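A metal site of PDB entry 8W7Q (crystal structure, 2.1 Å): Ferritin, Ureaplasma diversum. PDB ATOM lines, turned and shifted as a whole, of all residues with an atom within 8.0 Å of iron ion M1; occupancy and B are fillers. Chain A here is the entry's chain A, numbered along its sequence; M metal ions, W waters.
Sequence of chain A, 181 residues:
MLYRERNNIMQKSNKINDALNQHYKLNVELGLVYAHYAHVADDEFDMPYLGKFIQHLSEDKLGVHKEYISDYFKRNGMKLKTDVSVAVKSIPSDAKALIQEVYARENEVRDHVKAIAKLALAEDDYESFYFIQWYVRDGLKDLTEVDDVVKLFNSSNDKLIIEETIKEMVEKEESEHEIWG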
ATOM      1  N   ASN A  27     -26.718  -7.505  20.147  1.00  0.00           N
ATOM      2  CA  ASN A  27     -25.515  -6.697  20.334  1.00  0.00           C
ATOM      3  C   ASN A  27     -24.979  -6.192  19.002  1.00  0.00           C
ATOM      4  O   ASN A  27     -24.451  -5.073  18.930  1.00  0.00           O
ATOM      5  CB  ASN A  27     -24.458  -7.504  21.071  1.00  0.00           C
ATOM      6  CG  ASN A  27     -24.654  -7.443  22.566  1.00  0.00           C
ATOM      7  OD1 ASN A  27     -24.440  -6.408  23.182  1.00  0.00           O
ATOM      8  ND2 ASN A  27     -25.089  -8.559  23.155  1.00  0.00           N
ATOM      9  N   HIS A  56     -18.061   4.673  21.702  1.00  0.00           N
ATOM     10  CA  HIS A  56     -17.398   3.699  22.518  1.00  0.00           C
ATOM     11  C   HIS A  56     -18.353   2.585  22.882  1.00  0.00           C
ATOM     12  O   HIS A  56     -18.001   1.452  22.833  1.00  0.00           O
ATOM     13  CB  HIS A  56     -16.737   4.340  23.721  1.00  0.00           C
ATOM     14  CG  HIS A  56     -15.625   5.278  23.374  1.00  0.00           C
ATOM     15  ND1 HIS A  56     -15.014   5.302  22.140  1.00  0.00           N
ATOM     16  CD2 HIS A  56     -15.012   6.234  24.109  1.00  0.00           C
ATOM     17  CE1 HIS A  56     -14.082   6.231  22.135  1.00  0.00           C
ATOM     18  NE2 HIS A  56     -14.057   6.810  23.313  1.00  0.00           N
ATOM     19  N   LEU A  57     -19.576   2.934  23.219  1.00  0.00           N
ATOM     20  CA  LEU A  57     -20.593   1.944  23.474  1.00  0.00           C
ATOM     21  C   LEU A  57     -20.881   1.129  22.249  1.00  0.00           C
ATOM     22  O   LEU A  57     -21.058  -0.047  22.350  1.00  0.00           O
ATOM     23  CB  LEU A  57     -21.844   2.622  23.972  1.00  0.00           C
ATOM     24  CG  LEU A  57     -22.867   1.819  24.753  1.00  0.00           C
ATOM     25  CD1 LEU A  57     -22.240   1.150  25.958  1.00  0.00           C
ATOM     26  CD2 LEU A  57     -23.972   2.770  25.176  1.00  0.00           C
ATOM     27  N   GLU A  59     -18.741   0.322  19.895  1.00  0.00           N
ATOM     28  CA  GLU A  59     -17.628  -0.611  19.756  1.00  0.00           C
ATOM     29  C   GLU A  59     -17.615  -1.666  20.861  1.00  0.00           C
ATOM     30  O   GLU A  59     -17.103  -2.776  20.654  1.00  0.00           O
ATOM     31  CB  GLU A  59     -16.327   0.184  19.765  1.00  0.00           C
ATOM     32  CG  GLU A  59     -16.173   1.033  18.502  1.00  0.00           C
ATOM     33  CD  GLU A  59     -15.164   2.160  18.646  1.00  0.00           C
ATOM     34  OE1 GLU A  59     -15.064   2.980  17.713  1.00  0.00           O
ATOM     35  OE2 GLU A  59     -14.482   2.214  19.679  1.00  0.00           O
ATOM     36  N   ASP A  60     -18.142  -1.333  22.035  1.00  0.00           N
ATOM     37  CA  ASP A  60     -18.319  -2.304  23.104  1.00  0.00           C
ATOM     38  C   ASP A  60     -19.301  -3.400  22.696  1.00  0.00           C
ATOM     39  O   ASP A  60     -19.034  -4.599  22.868  1.00  0.00           O
ATOM     40  CB  ASP A  60     -18.778  -1.538  24.354  1.00  0.00           C
ATOM     41  CG  ASP A  60     -19.006  -2.407  25.564  1.00  0.00           C
ATOM     42  OD1 ASP A  60     -18.157  -3.279  25.862  1.00  0.00           O
ATOM     43  OD2 ASP A  60     -20.032  -2.168  26.242  1.00  0.00           O
ATOM     44  N   LYS A  61     -20.451  -3.015  22.125  1.00  0.00           N
ATOM     45  CA  LYS A  61     -21.450  -4.009  21.733  1.00  0.00           C
ATOM     46  C   LYS A  61     -20.957  -4.851  20.562  1.00  0.00           C
ATOM     47  O   LYS A  61     -21.121  -6.085  20.559  1.00  0.00           O
ATOM     48  CB  LYS A  61     -22.777  -3.342  21.348  1.00  0.00           C
ATOM     49  CG  LYS A  61     -23.382  -2.409  22.396  1.00  0.00           C
ATOM     50  CD  LYS A  61     -23.603  -3.114  23.718  1.00  0.00           C
ATOM     51  CE  LYS A  61     -24.284  -2.182  24.723  1.00  0.00           C
ATOM     52  NZ  LYS A  61     -24.620  -2.877  25.994  1.00  0.00           N
ATOM     53  N   VAL A  64     -16.506  -7.034  22.514  1.00  0.00           N
ATOM     54  CA  VAL A  64     -16.490  -8.155  23.459  1.00  0.00           C
ATOM     55  C   VAL A  64     -17.891  -8.732  23.677  1.00  0.00           C
ATOM     56  O   VAL A  64     -18.044  -9.935  23.869  1.00  0.00           O
ATOM     57  CB  VAL A  64     -15.851  -7.734  24.805  1.00  0.00           C
ATOM     58  CG1 VAL A  64     -14.376  -7.390  24.587  1.00  0.00           C
ATOM     59  CG2 VAL A  64     -16.638  -6.600  25.485  1.00  0.00           C
ATOM     60  N   HIS A  65     -18.929  -7.876  23.664  1.00  0.00           N
ATOM     61  CA  HIS A  65     -20.280  -8.393  23.913  1.00  0.00           C
ATOM     62  C   HIS A  65     -20.643  -9.495  22.930  1.00  0.00           C
ATOM     63  O   HIS A  65     -21.208 -10.523  23.324  1.00  0.00           O
ATOM     64  CB  HIS A  65     -21.308  -7.266  23.820  1.00  0.00           C
ATOM     65  CG  HIS A  65     -21.393  -6.389  25.023  1.00  0.00           C
ATOM     66  ND1 HIS A  65     -22.391  -6.495  25.960  1.00  0.00           N
ATOM     67  CD2 HIS A  65     -20.609  -5.351  25.430  1.00  0.00           C
ATOM     68  CE1 HIS A  65     -22.228  -5.573  26.893  1.00  0.00           C
ATOM     69  NE2 HIS A  65     -21.149  -4.868  26.590  1.00  0.00           N
ATOM     70  N   GLU A 106     -30.566   0.070  26.620  1.00  0.00           N
ATOM     71  CA  GLU A 106     -29.746  -0.609  27.624  1.00  0.00           C
ATOM     72  C   GLU A 106     -30.611  -1.225  28.714  1.00  0.00           C
ATOM     73  O   GLU A 106     -30.281  -2.283  29.241  1.00  0.00           O
ATOM     74  CB  GLU A 106     -28.738   0.355  28.259  1.00  0.00           C
ATOM     75  CG  GLU A 106     -27.630   0.832  27.315  1.00  0.00           C
ATOM     76  CD  GLU A 106     -26.841  -0.309  26.694  1.00  0.00           C
ATOM     77  OE1 GLU A 106     -26.358  -1.186  27.437  1.00  0.00           O
ATOM     78  OE2 GLU A 106     -26.692  -0.310  25.462  1.00  0.00           O
ATOM     79  N   VAL A 109     -31.640  -4.428  27.544  1.00  0.00           N
ATOM     80  CA  VAL A 109     -30.543  -5.399  27.621  1.00  0.00           C
ATOM     81  C   VAL A 109     -30.580  -6.114  28.972  1.00  0.00           C
ATOM     82  O   VAL A 109     -30.506  -7.355  29.032  1.00  0.00           O
ATOM     83  CB  VAL A 109     -29.186  -4.712  27.390  1.00  0.00           C
ATOM     84  CG1 VAL A 109     -28.045  -5.614  27.907  1.00  0.00           C
ATOM     85  CG2 VAL A 109     -28.999  -4.368  25.913  1.00  0.00           C
ATOM     86  N   TRP A 134     -21.100 -12.328  33.592  1.00  0.00           N
ATOM     87  CA  TRP A 134     -20.441 -11.173  32.979  1.00  0.00           C
ATOM     88  C   TRP A 134     -21.474 -10.197  32.425  1.00  0.00           C
ATOM     89  O   TRP A 134     -21.370  -8.982  32.627  1.00  0.00           O
ATOM     90  CB  TRP A 134     -19.484 -11.644  31.877  1.00  0.00           C
ATOM     91  CG  TRP A 134     -18.643 -10.558  31.354  1.00  0.00           C
ATOM     92  CD1 TRP A 134     -17.383 -10.220  31.773  1.00  0.00           C
ATOM     93  CD2 TRP A 134     -18.977  -9.640  30.300  1.00  0.00           C
ATOM     94  NE1 TRP A 134     -16.911  -9.144  31.040  1.00  0.00           N
ATOM     95  CE2 TRP A 134     -17.870  -8.770  30.131  1.00  0.00           C
ATOM     96  CE3 TRP A 134     -20.103  -9.471  29.474  1.00  0.00           C
ATOM     97  CZ2 TRP A 134     -17.862  -7.736  29.181  1.00  0.00           C
ATOM     98  CZ3 TRP A 134     -20.083  -8.436  28.517  1.00  0.00           C
ATOM     99  CH2 TRP A 134     -18.971  -7.595  28.382  1.00  0.00           C
ATOM    100  N   TYR A 135     -22.470 -10.730  31.709  1.00  0.00           N
ATOM    101  CA  TYR A 135     -23.502  -9.894  31.110  1.00  0.00           C
ATOM    102  C   TYR A 135     -24.459  -9.346  32.147  1.00  0.00           C
ATOM    103  O   TYR A 135     -25.004  -8.255  31.962  1.00  0.00           O
ATOM    104  CB  TYR A 135     -24.253 -10.689  30.037  1.00  0.00           C
ATOM    105  CG  TYR A 135     -23.374 -11.016  28.844  1.00  0.00           C
ATOM    106  CD1 TYR A 135     -22.413 -12.015  28.914  1.00  0.00           C
ATOM    107  CD2 TYR A 135     -23.495 -10.298  27.667  1.00  0.00           C
ATOM    108  CE1 TYR A 135     -21.599 -12.321  27.818  1.00  0.00           C
ATOM    109  CE2 TYR A 135     -22.687 -10.593  26.577  1.00  0.00           C
ATOM    110  CZ  TYR A 135     -21.741 -11.597  26.662  1.00  0.00           C
ATOM    111  OH  TYR A 135     -20.924 -11.896  25.572  1.00  0.00           O
ATOM    112  N   ARG A 137     -23.527  -8.454  35.250  1.00  0.00           N
ATOM    113  CA  ARG A 137     -22.770  -7.317  35.769  1.00  0.00           C
ATOM    114  C   ARG A 137     -22.728  -6.185  34.742  1.00  0.00           C
ATOM    115  O   ARG A 137     -22.972  -5.013  35.078  1.00  0.00           O
ATOM    116  CB  ARG A 137     -21.347  -7.753  36.144  1.00  0.00           C
ATOM    117  CG  ARG A 137     -20.477  -6.594  36.658  1.00  0.00           C
ATOM    118  CD  ARG A 137     -18.985  -6.841  36.400  1.00  0.00           C
ATOM    119  NE  ARG A 137     -18.713  -7.267  35.024  1.00  0.00           N
ATOM    120  CZ  ARG A 137     -18.707  -6.455  33.964  1.00  0.00           C
ATOM    121  NH1 ARG A 137     -18.960  -5.157  34.090  1.00  0.00           N
ATOM    122  NH2 ARG A 137     -18.461  -6.947  32.759  1.00  0.00           N
ATOM    123  N   ASP A 138     -22.453  -6.517  33.485  1.00  0.00           N
ATOM    124  CA  ASP A 138     -22.272  -5.457  32.506  1.00  0.00           C
ATOM    125  C   ASP A 138     -23.582  -4.749  32.164  1.00  0.00           C
ATOM    126  O   ASP A 138     -23.572  -3.569  31.805  1.00  0.00           O
ATOM    127  CB  ASP A 138     -21.627  -6.015  31.244  1.00  0.00           C
ATOM    128  CG  ASP A 138     -20.839  -4.961  30.497  1.00  0.00           C
ATOM    129  OD1 ASP A 138     -19.816  -4.492  31.038  1.00  0.00           O
ATOM    130  OD2 ASP A 138     -21.247  -4.597  29.390  1.00  0.00           O
ATOM    131  N   GLY A 139     -24.698  -5.453  32.244  1.00  0.00           N
ATOM    132  CA  GLY A 139     -25.974  -4.791  32.011  1.00  0.00           C
ATOM    133  C   GLY A 139     -26.168  -3.586  32.902  1.00  0.00           C
ATOM    134  O   GLY A 139     -26.616  -2.523  32.455  1.00  0.00           O
ATOM    135  N   LYS A 141     -23.611  -2.027  34.724  1.00  0.00           N
ATOM    136  CA  LYS A 141     -22.539  -1.057  34.516  1.00  0.00           C
ATOM    137  C   LYS A 141     -22.836  -0.154  33.320  1.00  0.00           C
ATOM    138  O   LYS A 141     -22.774   1.073  33.426  1.00  0.00           O
ATOM    139  CB  LYS A 141     -21.201  -1.751  34.337  1.00  0.00           C
ATOM    140  CG  LYS A 141     -20.055  -0.746  34.386  1.00  0.00           C
ATOM    141  CD  LYS A 141     -19.110  -0.846  33.244  1.00  0.00           C
ATOM    142  CE  LYS A 141     -17.788  -0.191  33.631  1.00  0.00           C
ATOM    143  NZ  LYS A 141     -16.607  -0.731  32.907  1.00  0.00           N
ATOM    144  N   ASP A 142     -23.158  -0.760  32.171  1.00  0.00           N
ATOM    145  CA  ASP A 142     -23.448   0.044  30.980  1.00  0.00           C
ATOM    146  C   ASP A 142     -24.618   0.990  31.203  1.00  0.00           C
ATOM    147  O   ASP A 142     -24.579   2.151  30.782  1.00  0.00           O
ATOM    148  CB  ASP A 142     -23.724  -0.876  29.796  1.00  0.00           C
ATOM    149  CG  ASP A 142     -22.458  -1.433  29.167  1.00  0.00           C
ATOM    150  OD1 ASP A 142     -21.370  -0.993  29.569  1.00  0.00           O
ATOM    151  OD2 ASP A 142     -22.569  -2.327  28.308  1.00  0.00           O
ATOM    152  N   LEU A 143     -25.685   0.499  31.847  1.00  0.00           N
ATOM    153  CA  LEU A 143     -26.827   1.377  32.126  1.00  0.00           C
ATOM    154  C   LEU A 143     -26.404   2.555  32.993  1.00  0.00           C
ATOM    155  O   LEU A 143     -26.818   3.696  32.754  1.00  0.00           O
ATOM    156  CB  LEU A 143     -27.947   0.591  32.818  1.00  0.00           C
ATOM    157  CG  LEU A 143     -29.201   1.435  33.033  1.00  0.00           C
ATOM    158  CD1 LEU A 143     -30.117   1.379  31.823  1.00  0.00           C
ATOM    159  CD2 LEU A 143     -29.952   1.027  34.291  1.00  0.00           C
ATOM    160  N   GLU A 145     -23.495   3.941  33.204  1.00  0.00           N
ATOM    161  CA  GLU A 145     -22.692   4.891  32.462  1.00  0.00           C
ATOM    162  C   GLU A 145     -23.573   5.756  31.582  1.00  0.00           C
ATOM    163  O   GLU A 145     -23.392   6.969  31.517  1.00  0.00           O
ATOM    164  CB  GLU A 145     -21.617   4.171  31.650  1.00  0.00           C
ATOM    165  CG  GLU A 145     -20.512   3.640  32.558  1.00  0.00           C
ATOM    166  CD  GLU A 145     -19.476   2.811  31.825  1.00  0.00           C
ATOM    167  OE1 GLU A 145     -19.749   2.329  30.696  1.00  0.00           O
ATOM    168  OE2 GLU A 145     -18.373   2.620  32.396  1.00  0.00           O
HETATM  169 FE    FE M   1     -20.648  -3.344  27.953  1.00  0.00          FE
HETATM  170 FE    FE M   2     -16.136   1.281  29.148  1.00  0.00          FE
HETATM  171  O   HOH W   1     -18.641  -3.631  28.546  1.00  0.00           O
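The side-chain amide oxygen (OD1) of Asn 27 lies close to a ring nitrogen (ND1) of His 65 (3.5 Å).
The side-chain carboxylate (OD1) of Asp 138 is in salt-bridge range of the guanidinium group (NH1) of Arg 137 (3.2 Å).
OD2 of Asp 142 lies close to NZ of Lys 61.
The backbone carbonyl oxygen (O) of His 65 lies within hydrogen-bond range of the side-chain hydroxyl (OH) of Tyr 135, 2.6 Å away.
OD2 of Asp 138 is bound to iron ion M1 (2.0 Å).
Iron ion M1 is bound by a ring nitrogen (NE2) of His 65 (2.1 Å).
Iron ion M1 is bound by water W1 (2.1 Å).
Iron ion M1 is bound by the side-chain carboxylate (OD2) of Asp 60, at 2.2 Å.
The side-chain carboxylate (OD2) of Asp 142 binds iron ion M1 (2.2 Å).
Iron ion M1 has five donor atoms within binding distance.
Water W1 lies within hydrogen-bond range of the side-chain carboxylate of Asp 60 (2.7 Å) and the side-chain carboxylate of Asp 138 (2.9 Å).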
